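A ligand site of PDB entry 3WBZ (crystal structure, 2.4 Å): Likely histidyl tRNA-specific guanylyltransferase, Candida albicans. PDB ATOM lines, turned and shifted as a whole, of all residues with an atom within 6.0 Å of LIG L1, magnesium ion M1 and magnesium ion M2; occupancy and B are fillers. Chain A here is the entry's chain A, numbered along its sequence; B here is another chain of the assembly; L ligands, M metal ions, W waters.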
ATOM      1  N   ASP A  32     -12.006 -35.667 -12.161  1.00  0.00           N
ATOM      2  CA  ASP A  32     -12.158 -34.306 -12.689  1.00  0.00           C
ATOM      3  C   ASP A  32     -12.722 -34.356 -14.097  1.00  0.00           C
ATOM      4  O   ASP A  32     -12.226 -35.102 -14.953  1.00  0.00           O
ATOM      5  CB  ASP A  32     -10.808 -33.578 -12.685  1.00  0.00           C
ATOM      6  CG  ASP A  32     -10.921 -32.159 -13.227  1.00  0.00           C
ATOM      7  OD1 ASP A  32     -11.049 -32.009 -14.447  1.00  0.00           O
ATOM      8  OD2 ASP A  32     -10.859 -31.193 -12.443  1.00  0.00           O
ATOM      9  N   GLY A  33     -13.726 -33.523 -14.358  1.00  0.00           N
ATOM     10  CA  GLY A  33     -14.405 -33.515 -15.637  1.00  0.00           C
ATOM     11  C   GLY A  33     -13.463 -33.213 -16.780  1.00  0.00           C
ATOM     12  O   GLY A  33     -12.680 -32.275 -16.732  1.00  0.00           O
ATOM     13  N   LYS A  34     -13.549 -34.003 -17.838  1.00  0.00           N
ATOM     14  CA  LYS A  34     -12.710 -33.808 -19.014  1.00  0.00           C
ATOM     15  C   LYS A  34     -13.275 -32.713 -19.937  1.00  0.00           C
ATOM     16  O   LYS A  34     -14.412 -32.818 -20.421  1.00  0.00           O
ATOM     17  CB  LYS A  34     -12.574 -35.118 -19.791  1.00  0.00           C
ATOM     18  CG  LYS A  34     -11.751 -34.986 -21.079  1.00  0.00           C
ATOM     19  CD  LYS A  34     -11.940 -36.191 -21.990  1.00  0.00           C
ATOM     20  CE  LYS A  34     -11.349 -35.896 -23.358  1.00  0.00           C
ATOM     21  NZ  LYS A  34      -9.931 -35.364 -23.217  1.00  0.00           N
ATOM     22  N   GLY A  35     -12.472 -31.674 -20.162  1.00  0.00           N
ATOM     23  CA  GLY A  35     -12.881 -30.577 -21.035  1.00  0.00           C
ATOM     24  C   GLY A  35     -14.154 -29.894 -20.568  1.00  0.00           C
ATOM     25  O   GLY A  35     -15.033 -29.572 -21.368  1.00  0.00           O
ATOM     26  N   PHE A  36     -14.273 -29.640 -19.276  1.00  0.00           N
ATOM     27  CA  PHE A  36     -15.484 -29.010 -18.786  1.00  0.00           C
ATOM     28  C   PHE A  36     -15.539 -27.514 -19.013  1.00  0.00           C
ATOM     29  O   PHE A  36     -16.593 -26.900 -18.813  1.00  0.00           O
ATOM     30  CB  PHE A  36     -15.683 -29.295 -17.311  1.00  0.00           C
ATOM     31  CG  PHE A  36     -16.698 -30.369 -17.047  1.00  0.00           C
ATOM     32  CD1 PHE A  36     -16.517 -31.643 -17.573  1.00  0.00           C
ATOM     33  CD2 PHE A  36     -17.846 -30.112 -16.284  1.00  0.00           C
ATOM     34  CE1 PHE A  36     -17.444 -32.664 -17.310  1.00  0.00           C
ATOM     35  CE2 PHE A  36     -18.773 -31.132 -16.022  1.00  0.00           C
ATOM     36  CZ  PHE A  36     -18.571 -32.405 -16.545  1.00  0.00           C
ATOM     37  N   HIS A  37     -14.436 -26.891 -19.439  1.00  0.00           N
ATOM     38  CA  HIS A  37     -14.564 -25.518 -19.901  1.00  0.00           C
ATOM     39  C   HIS A  37     -15.466 -25.519 -21.158  1.00  0.00           C
ATOM     40  O   HIS A  37     -16.443 -24.766 -21.221  1.00  0.00           O
ATOM     41  CB  HIS A  37     -13.214 -24.862 -20.192  1.00  0.00           C
ATOM     42  CG  HIS A  37     -13.335 -23.446 -20.642  1.00  0.00           C
ATOM     43  ND1 HIS A  37     -13.517 -22.401 -19.757  1.00  0.00           N
ATOM     44  CD2 HIS A  37     -13.412 -22.898 -21.877  1.00  0.00           C
ATOM     45  CE1 HIS A  37     -13.644 -21.272 -20.428  1.00  0.00           C
ATOM     46  NE2 HIS A  37     -13.594 -21.551 -21.718  1.00  0.00           N
ATOM     47  N   LYS A  38     -15.153 -26.338 -22.170  1.00  0.00           N
ATOM     48  CA  LYS A  38     -16.016 -26.440 -23.354  1.00  0.00           C
ATOM     49  C   LYS A  38     -17.405 -26.948 -23.052  1.00  0.00           C
ATOM     50  O   LYS A  38     -18.398 -26.447 -23.588  1.00  0.00           O
ATOM     51  CB  LYS A  38     -15.450 -27.351 -24.451  1.00  0.00           C
ATOM     52  CG  LYS A  38     -14.299 -26.789 -25.268  1.00  0.00           C
ATOM     53  CD  LYS A  38     -13.880 -27.798 -26.339  1.00  0.00           C
ATOM     54  CE  LYS A  38     -12.685 -27.318 -27.148  1.00  0.00           C
ATOM     55  NZ  LYS A  38     -12.260 -28.332 -28.182  1.00  0.00           N
ATOM     56  N   SER A  40     -19.104 -26.591 -20.347  1.00  0.00           N
ATOM     57  CA  SER A  40     -19.878 -25.537 -19.709  1.00  0.00           C
ATOM     58  C   SER A  40     -20.278 -24.423 -20.689  1.00  0.00           C
ATOM     59  O   SER A  40     -21.256 -23.734 -20.486  1.00  0.00           O
ATOM     60  CB  SER A  40     -19.110 -24.950 -18.522  1.00  0.00           C
ATOM     61  OG  SER A  40     -17.980 -24.227 -18.965  1.00  0.00           O
ATOM     62  N   PHE A  45     -23.662 -22.933 -19.219  1.00  0.00           N
ATOM     63  CA  PHE A  45     -23.639 -22.791 -17.766  1.00  0.00           C
ATOM     64  C   PHE A  45     -23.707 -21.314 -17.389  1.00  0.00           C
ATOM     65  O   PHE A  45     -23.107 -20.471 -18.043  1.00  0.00           O
ATOM     66  CB  PHE A  45     -22.347 -23.388 -17.156  1.00  0.00           C
ATOM     67  CG  PHE A  45     -22.318 -24.892 -17.087  1.00  0.00           C
ATOM     68  CD1 PHE A  45     -23.121 -25.680 -17.890  1.00  0.00           C
ATOM     69  CD2 PHE A  45     -21.494 -25.529 -16.169  1.00  0.00           C
ATOM     70  CE1 PHE A  45     -23.078 -27.064 -17.819  1.00  0.00           C
ATOM     71  CE2 PHE A  45     -21.442 -26.926 -16.082  1.00  0.00           C
ATOM     72  CZ  PHE A  45     -22.242 -27.694 -16.922  1.00  0.00           C
ATOM     73  N   GLU A  46     -24.403 -20.991 -16.318  1.00  0.00           N
ATOM     74  CA  GLU A  46     -24.281 -19.658 -15.738  1.00  0.00           C
ATOM     75  C   GLU A  46     -22.848 -19.446 -15.240  1.00  0.00           C
ATOM     76  O   GLU A  46     -22.158 -20.362 -14.797  1.00  0.00           O
ATOM     77  CB  GLU A  46     -25.258 -19.478 -14.579  1.00  0.00           C
ATOM     78  CG  GLU A  46     -26.705 -19.566 -14.993  1.00  0.00           C
ATOM     79  CD  GLU A  46     -27.640 -19.152 -13.877  1.00  0.00           C
ATOM     80  OE1 GLU A  46     -27.146 -18.567 -12.878  1.00  0.00           O
ATOM     81  OE2 GLU A  46     -28.870 -19.435 -14.012  1.00  0.00           O
ATOM     82  N   LYS A  47     -22.432 -18.190 -15.312  1.00  0.00           N
ATOM     83  CA  LYS A  47     -21.114 -17.809 -14.867  1.00  0.00           C
ATOM     84  C   LYS A  47     -21.295 -16.760 -13.776  1.00  0.00           C
ATOM     85  O   LYS A  47     -22.215 -15.962 -13.836  1.00  0.00           O
ATOM     86  CB  LYS A  47     -20.310 -17.283 -16.056  1.00  0.00           C
ATOM     87  CG  LYS A  47     -20.081 -18.342 -17.113  1.00  0.00           C
ATOM     88  CD  LYS A  47     -19.181 -19.462 -16.549  1.00  0.00           C
ATOM     89  CE  LYS A  47     -18.903 -20.539 -17.580  1.00  0.00           C
ATOM     90  NZ  LYS A  47     -17.751 -21.380 -17.184  1.00  0.00           N
ATOM     91  N   PRO A  48     -20.411 -16.773 -12.763  1.00  0.00           N
ATOM     92  CA  PRO A  48     -19.264 -17.676 -12.598  1.00  0.00           C
ATOM     93  C   PRO A  48     -19.663 -19.097 -12.175  1.00  0.00           C
ATOM     94  O   PRO A  48     -18.961 -20.034 -12.534  1.00  0.00           O
ATOM     95  CB  PRO A  48     -18.431 -17.000 -11.516  1.00  0.00           C
ATOM     96  CG  PRO A  48     -19.458 -16.223 -10.696  1.00  0.00           C
ATOM     97  CD  PRO A  48     -20.479 -15.755 -11.681  1.00  0.00           C
ATOM     98  N   ASN A  49     -20.730 -19.233 -11.414  1.00  0.00           N
ATOM     99  CA  ASN A  49     -21.149 -20.559 -10.933  1.00  0.00           C
ATOM    100  C   ASN A  49     -22.550 -20.942 -11.357  1.00  0.00           C
ATOM    101  O   ASN A  49     -23.505 -20.178 -11.219  1.00  0.00           O
ATOM    102  CB  ASN A  49     -21.062 -20.623  -9.408  1.00  0.00           C
ATOM    103  CG  ASN A  49     -19.654 -20.341  -8.900  1.00  0.00           C
ATOM    104  OD1 ASN A  49     -18.740 -21.120  -9.133  1.00  0.00           O
ATOM    105  ND2 ASN A  49     -19.495 -19.245  -8.157  1.00  0.00           N
ATOM    106  N   ASP A  50     -22.672 -22.153 -11.892  1.00  0.00           N
ATOM    107  CA  ASP A  50     -23.983 -22.677 -12.223  1.00  0.00           C
ATOM    108  C   ASP A  50     -24.431 -23.587 -11.096  1.00  0.00           C
ATOM    109  O   ASP A  50     -23.872 -24.671 -10.892  1.00  0.00           O
ATOM    110  CB  ASP A  50     -23.957 -23.426 -13.549  1.00  0.00           C
ATOM    111  CG  ASP A  50     -25.342 -23.709 -14.082  1.00  0.00           C
ATOM    112  OD1 ASP A  50     -26.061 -24.524 -13.462  1.00  0.00           O
ATOM    113  OD2 ASP A  50     -25.709 -23.142 -15.125  1.00  0.00           O
ATOM    114  N   LEU A  51     -25.433 -23.148 -10.364  1.00  0.00           N
ATOM    115  CA  LEU A  51     -25.897 -23.843  -9.179  1.00  0.00           C
ATOM    116  C   LEU A  51     -26.372 -25.256  -9.481  1.00  0.00           C
ATOM    117  O   LEU A  51     -25.952 -26.208  -8.813  1.00  0.00           O
ATOM    118  CB  LEU A  51     -27.004 -23.043  -8.503  1.00  0.00           C
ATOM    119  CG  LEU A  51     -27.750 -23.776  -7.391  1.00  0.00           C
ATOM    120  CD1 LEU A  51     -26.819 -24.149  -6.256  1.00  0.00           C
ATOM    121  CD2 LEU A  51     -28.887 -22.921  -6.856  1.00  0.00           C
ATOM    122  N   ALA A  53     -25.681 -27.108 -11.993  1.00  0.00           N
ATOM    123  CA  ALA A  53     -24.554 -27.896 -12.455  1.00  0.00           C
ATOM    124  C   ALA A  53     -23.779 -28.464 -11.261  1.00  0.00           C
ATOM    125  O   ALA A  53     -23.336 -29.602 -11.300  1.00  0.00           O
ATOM    126  CB  ALA A  53     -23.661 -27.067 -13.351  1.00  0.00           C
ATOM    127  N   LEU A  54     -23.612 -27.671 -10.210  1.00  0.00           N
ATOM    128  CA  LEU A  54     -22.984 -28.152  -8.984  1.00  0.00           C
ATOM    129  C   LEU A  54     -23.874 -29.160  -8.250  1.00  0.00           C
ATOM    130  O   LEU A  54     -23.382 -30.103  -7.611  1.00  0.00           O
ATOM    131  CB  LEU A  54     -22.623 -26.988  -8.062  1.00  0.00           C
ATOM    132  CG  LEU A  54     -21.446 -26.124  -8.550  1.00  0.00           C
ATOM    133  CD1 LEU A  54     -21.295 -24.887  -7.679  1.00  0.00           C
ATOM    134  CD2 LEU A  54     -20.153 -26.921  -8.512  1.00  0.00           C
ATOM    135  N   ASP A  77     -15.675 -29.385  -5.739  1.00  0.00           N
ATOM    136  CA  ASP A  77     -15.953 -28.025  -6.193  1.00  0.00           C
ATOM    137  C   ASP A  77     -15.671 -27.964  -7.692  1.00  0.00           C
ATOM    138  O   ASP A  77     -14.899 -28.792  -8.206  1.00  0.00           O
ATOM    139  CB  ASP A  77     -15.085 -27.025  -5.451  1.00  0.00           C
ATOM    140  CG  ASP A  77     -13.675 -27.035  -5.924  1.00  0.00           C
ATOM    141  OD1 ASP A  77     -12.960 -27.981  -5.521  1.00  0.00           O
ATOM    142  OD2 ASP A  77     -13.263 -26.113  -6.663  1.00  0.00           O
ATOM    143  N   SER A  78     -16.279 -27.008  -8.392  1.00  0.00           N
ATOM    144  CA  SER A  78     -16.074 -26.904  -9.828  1.00  0.00           C
ATOM    145  C   SER A  78     -16.420 -28.245 -10.492  1.00  0.00           C
ATOM    146  O   SER A  78     -17.498 -28.793 -10.266  1.00  0.00           O
ATOM    147  CB  SER A  78     -14.640 -26.473 -10.143  1.00  0.00           C
ATOM    148  OG  SER A  78     -14.460 -26.348 -11.547  1.00  0.00           O
ATOM    149  N   ASP A  79     -15.505 -28.778 -11.312  1.00  0.00           N
ATOM    150  CA  ASP A  79     -15.774 -30.066 -11.964  1.00  0.00           C
ATOM    151  C   ASP A  79     -15.038 -31.253 -11.320  1.00  0.00           C
ATOM    152  O   ASP A  79     -14.797 -32.255 -11.988  1.00  0.00           O
ATOM    153  CB  ASP A  79     -15.403 -29.992 -13.448  1.00  0.00           C
ATOM    154  CG  ASP A  79     -13.898 -29.915 -13.675  1.00  0.00           C
ATOM    155  OD1 ASP A  79     -13.211 -29.465 -12.738  1.00  0.00           O
ATOM    156  OD2 ASP A  79     -13.417 -30.306 -14.778  1.00  0.00           O
ATOM    157  N   GLU A  80     -14.676 -31.161 -10.032  1.00  0.00           N
ATOM    158  CA  GLU A  80     -13.887 -32.218  -9.389  1.00  0.00           C
ATOM    159  C   GLU A  80     -14.521 -32.724  -8.093  1.00  0.00           C
ATOM    160  O   GLU A  80     -15.260 -32.014  -7.428  1.00  0.00           O
ATOM    161  CB  GLU A  80     -12.438 -31.734  -9.115  1.00  0.00           C
ATOM    162  CG  GLU A  80     -12.221 -31.092  -7.754  1.00  0.00           C
ATOM    163  CD  GLU A  80     -10.779 -30.630  -7.501  1.00  0.00           C
ATOM    164  OE1 GLU A  80     -10.162 -30.035  -8.433  1.00  0.00           O
ATOM    165  OE2 GLU A  80     -10.279 -30.844  -6.349  1.00  0.00           O
ATOM    166  N   ASN A 163     -12.705 -16.318 -10.508  1.00  0.00           N
ATOM    167  CA  ASN A 163     -13.787 -16.433 -11.484  1.00  0.00           C
ATOM    168  C   ASN A 163     -14.927 -15.477 -11.195  1.00  0.00           C
ATOM    169  O   ASN A 163     -15.525 -14.922 -12.124  1.00  0.00           O
ATOM    170  CB  ASN A 163     -14.355 -17.857 -11.531  1.00  0.00           C
ATOM    171  CG  ASN A 163     -13.388 -18.837 -12.120  1.00  0.00           C
ATOM    172  OD1 ASN A 163     -12.587 -18.469 -12.966  1.00  0.00           O
ATOM    173  ND2 ASN A 163     -13.492 -20.096 -11.712  1.00  0.00           N
ATOM    174  N   LYS B  98      -4.861 -42.185 -17.440  1.00  0.00           N
ATOM    175  CA  LYS B  98      -5.693 -41.413 -18.343  1.00  0.00           C
ATOM    176  C   LYS B  98      -6.408 -42.282 -19.405  1.00  0.00           C
ATOM    177  O   LYS B  98      -7.589 -42.101 -19.672  1.00  0.00           O
ATOM    178  CB  LYS B  98      -4.860 -40.342 -19.037  1.00  0.00           C
ATOM    179  CG  LYS B  98      -4.466 -39.184 -18.132  1.00  0.00           C
ATOM    180  CD  LYS B  98      -5.642 -38.260 -17.874  1.00  0.00           C
ATOM    181  CE  LYS B  98      -5.169 -37.029 -17.115  1.00  0.00           C
ATOM    182  NZ  LYS B  98      -6.255 -36.052 -16.872  1.00  0.00           N
HETATM  183  P1  LIG L   1      -9.313 -30.792 -18.114  1.00  0.00           P
HETATM  184  O1  LIG L   1      -7.834 -30.509 -18.062  1.00  0.00           O
HETATM  185  O2  LIG L   1      -9.944 -31.068 -16.759  1.00  0.00           O
HETATM  186  O3  LIG L   1      -9.678 -31.746 -19.225  1.00  0.00           O
HETATM  187  P2  LIG L   1     -11.182 -28.595 -18.003  1.00  0.00           P
HETATM  188  O4  LIG L   1     -11.688 -27.735 -19.122  1.00  0.00           O
HETATM  189  O5  LIG L   1     -12.153 -29.518 -17.315  1.00  0.00           O
HETATM  190  O6  LIG L   1      -9.903 -29.370 -18.608  1.00  0.00           O
HETATM  191  P3  LIG L   1     -10.549 -27.596 -15.327  1.00  0.00           P
HETATM  192  O7  LIG L   1      -9.339 -27.031 -14.667  1.00  0.00           O
HETATM  193  O8  LIG L   1     -11.084 -28.910 -14.786  1.00  0.00           O
HETATM  194  O9  LIG L   1     -10.391 -27.638 -16.938  1.00  0.00           O
HETATM  195  O10 LIG L   1     -11.696 -26.482 -15.260  1.00  0.00           O
HETATM  196  C1  LIG L   1     -13.101 -26.765 -15.241  1.00  0.00           C
HETATM  197  C2  LIG L   1     -13.870 -25.577 -15.846  1.00  0.00           C
HETATM  198  O11 LIG L   1     -15.246 -25.889 -16.136  1.00  0.00           O
HETATM  199  C3  LIG L   1     -13.912 -24.348 -14.950  1.00  0.00           C
HETATM  200  O12 LIG L   1     -12.798 -23.487 -15.187  1.00  0.00           O
HETATM  201  C4  LIG L   1     -15.151 -23.649 -15.425  1.00  0.00           C
HETATM  202  O13 LIG L   1     -14.735 -22.978 -16.621  1.00  0.00           O
HETATM  203  C5  LIG L   1     -16.080 -24.744 -15.892  1.00  0.00           C
HETATM  204  N1  LIG L   1     -17.068 -25.131 -14.855  1.00  0.00           N
HETATM  205  C6  LIG L   1     -17.072 -26.319 -14.257  1.00  0.00           C
HETATM  206  N2  LIG L   1     -18.101 -26.412 -13.388  1.00  0.00           N
HETATM  207  C7  LIG L   1     -18.787 -25.262 -13.444  1.00  0.00           C
HETATM  208  C8  LIG L   1     -19.990 -24.715 -12.785  1.00  0.00           C
HETATM  209  N3  LIG L   1     -20.667 -25.457 -11.880  1.00  0.00           N
HETATM  210  N4  LIG L   1     -20.382 -23.482 -13.130  1.00  0.00           N
HETATM  211  C9  LIG L   1     -19.732 -22.771 -14.050  1.00  0.00           C
HETATM  212  N5  LIG L   1     -18.648 -23.202 -14.690  1.00  0.00           N
HETATM  213  C10 LIG L   1     -18.118 -24.426 -14.425  1.00  0.00           C
HETATM  214  P1  LG2 L   2      -3.355 -34.033 -15.372  1.00  0.00           P
HETATM  215  O1  LG2 L   2      -2.747 -35.026 -14.422  1.00  0.00           O
HETATM  216  O2  LG2 L   2      -4.863 -33.903 -15.227  1.00  0.00           O
HETATM  217  O3  LG2 L   2      -2.842 -34.086 -16.801  1.00  0.00           O
HETATM  218  P2  LG2 L   2      -3.460 -31.286 -14.400  1.00  0.00           P
HETATM  219  O4  LG2 L   2      -2.486 -30.133 -14.472  1.00  0.00           O
HETATM  220  O5  LG2 L   2      -4.818 -31.119 -15.038  1.00  0.00           O
HETATM  221  O6  LG2 L   2      -2.683 -32.611 -14.917  1.00  0.00           O
HETATM  222  P3  LG2 L   2      -4.801 -32.216 -11.940  1.00  0.00           P
HETATM  223  O7  LG2 L   2      -4.200 -33.191 -10.920  1.00  0.00           O
HETATM  224  O8  LG2 L   2      -5.966 -32.705 -12.799  1.00  0.00           O
HETATM  225  O9  LG2 L   2      -3.554 -31.646 -12.812  1.00  0.00           O
HETATM  226  O10 LG2 L   2      -5.301 -30.920 -11.125  1.00  0.00           O
HETATM  227  C1  LG2 L   2      -5.335 -30.988  -9.703  1.00  0.00           C
HETATM  228  C2  LG2 L   2      -4.801 -29.685  -9.106  1.00  0.00           C
HETATM  229  O11 LG2 L   2      -3.378 -29.757  -9.013  1.00  0.00           O
HETATM  230  C3  LG2 L   2      -5.125 -28.484  -9.976  1.00  0.00           C
HETATM  231  O12 LG2 L   2      -5.547 -27.423  -9.114  1.00  0.00           O
HETATM  232  C4  LG2 L   2      -3.805 -28.066 -10.578  1.00  0.00           C
HETATM  233  O13 LG2 L   2      -3.827 -26.647 -10.671  1.00  0.00           O
HETATM  234  C5  LG2 L   2      -2.795 -28.576  -9.564  1.00  0.00           C
HETATM  235  N1  LG2 L   2      -1.486 -28.973 -10.149  1.00  0.00           N
HETATM  236  C6  LG2 L   2      -1.299 -29.503 -11.364  1.00  0.00           C
HETATM  237  N2  LG2 L   2       0.011 -29.768 -11.586  1.00  0.00           N
HETATM  238  C7  LG2 L   2       0.688 -29.409 -10.489  1.00  0.00           C
HETATM  239  C8  LG2 L   2       2.108 -29.421 -10.058  1.00  0.00           C
HETATM  240  N3  LG2 L   2       3.060 -29.883 -10.893  1.00  0.00           N
HETATM  241  N4  LG2 L   2       2.396 -28.967  -8.824  1.00  0.00           N
HETATM  242  C9  LG2 L   2       1.443 -28.499  -7.996  1.00  0.00           C
HETATM  243  N5  LG2 L   2       0.133 -28.448  -8.319  1.00  0.00           N
HETATM  244  C10 LG2 L   2      -0.299 -28.880  -9.539  1.00  0.00           C
HETATM  245 MG    MG M   1     -11.126 -29.090 -12.656  1.00  0.00          MG
HETATM  246 MG    MG M   2     -11.583 -30.772 -15.794  1.00  0.00          MG
HETATM  247 MG    MG M   3      -6.323 -32.723 -14.843  1.00  0.00          MG
HETATM  248  O   HOH W   1     -18.183 -23.639 -10.338  1.00  0.00           O
HETATM  249  O   HOH W   2      -6.150 -29.196 -16.392  1.00  0.00           O
HETATM  250  O   HOH W   3     -12.291 -27.606 -22.327  1.00  0.00           O
HETATM  251  O   HOH W   4      -9.033 -28.802 -12.505  1.00  0.00           O
HETATM  252  O   HOH W   5     -19.636 -28.399 -11.976  1.00  0.00           O
HETATM  253  O   HOH W   6     -11.380 -26.857 -12.304  1.00  0.00           O
HETATM  254  O   HOH W   7     -11.212 -28.729 -10.456  1.00  0.00           O
HETATM  255  O   HOH W   8      -9.933 -34.062 -16.434  1.00  0.00           O
HETATM  256  O   HOH W   9      -7.943 -33.610 -19.919  1.00  0.00           O
HETATM  257  O   HOH W  10      -7.803 -31.392 -14.675  1.00  0.00           O
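OG of Ser 40 lies within hydrogen-bond range of O of His 37, 2.8 Å away. The side-chain hydroxyl of Ser 40 is in hydrogen-bond range of the side-chain amino group of Lys 47, at 3.4 Å. The backbone carbonyl oxygen (O) of Ser 40 is in hydrogen-bond range of the backbone NH (N) of Phe 45, 2.8 Å away. N of Ala 53 is in hydrogen-bond range of OD1 of Asp 50, at 3.0 Å. The side-chain hydroxyl (OG) of Ser 40 sits at hydrogen-bond distance from the backbone carbonyl oxygen (O) of Phe 36, 3.0 Å away. The side-chain carboxylate (OD2) of Asp 50 lies within hydrogen-bond range of the backbone NH (N) of Glu 46 (2.8 Å).
Magnesium ion M1 is bound by water W4 (2.1 Å), OD1 of Asp 79 (2.1 Å), OD2 of Asp 32 (2.1 Å), O8 of LIG L1 (2.1 Å), water W7 (2.2 Å) and water W6 (2.3 Å).
Magnesium ion M2 is bound by the side-chain carboxylate (OD1) of Asp 32 (1.9 Å), an oxygen (O2) of LIG L1 (1.9 Å), an oxygen (O5) of LIG L1 (2.1 Å), the backbone carbonyl oxygen (O) of Gly 33 (2.1 Å), the side-chain carboxylate (OD2) of Asp 79 (2.1 Å) and an oxygen (O8) of LIG L1 (2.2 Å).
Water W6 lies within hydrogen-bond range of O10 of LIG L1 and OG of Ser 78. Water W5 bridges the backbone carbonyl oxygen of Ser 78 (2.8 Å) and a nitrogen (N2) of LIG L1 (2.9 Å). Water W1 bridges the side-chain amide oxygen (OD1) of Asn 49 (2.8 Å) and a nitrogen (N3) of LIG L1 (3.4 Å). Water W3 bridges the backbone NH (N) of Lys 38 and an oxygen (O4) of LIG L1.
Of the 23 residues printed, 2 come within 4 Å of magnesium ion M1. Along chain A the residues within 4 Å of magnesium ion M1 span positions 32 to 79. The nearest printed residue that does not touch magnesium ion M1 is Glu 80 (4.4 Å).
Within 4 Å of magnesium ion M2: Asp 32, Gly 33 and Asp 79. Along chain A the residues within 4 Å of magnesium ion M2 span positions 32 to 79.
Residues that only touch LIG L1: Pro 48, Leu 54, Glu 46, Ser 40, Lys 34, Ala 53, Asn 49, Ser 78 and Phe 45. Hydrophobic or aromatic side chains that line LIG L1: Phe 36, His 37, Phe 45, Ala 53 and Leu 54. 17 residues have an atom within 4 Å of LIG L1: Asp 32, Gly 33, Lys 34, Gly 35, Phe 36, His 37, Ser 40, Phe 45, Glu 46, Lys 47, Pro 48, Asn 49, Asp 50, Ala 53, Leu 54, Ser 78 and Asp 79.
An oxygen (O3) of LIG L1 is in hydrogen-bond range of the backbone NH (N) of Gly 35 (2.9 Å). NZ of Lys 47 is in hydrogen-bond range of N5 of LIG L1, at 3.2 Å. O13 of LIG L1 is in hydrogen-bond range of ND1 of His 37, at 3.4 Å. N of His 37 is in hydrogen-bond range of O4 of LIG L1, at 2.9 Å. An oxygen (O3) of LG2 L2 lies within salt-bridge range of the side-chain amino group of Lys 98 of chain B, at 3.9 Å. The backbone carbonyl oxygen (O) of Asp 50 sits at hydrogen-bond distance from a nitrogen (N3) of LIG L1 (3.4 Å). O4 of LIG L1 sits at hydrogen-bond distance from N of Phe 36 (3.2 Å). A nitrogen (N4) of LIG L1 sits at hydrogen-bond distance from the backbone NH (N) of Asp 50 (2.9 Å).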
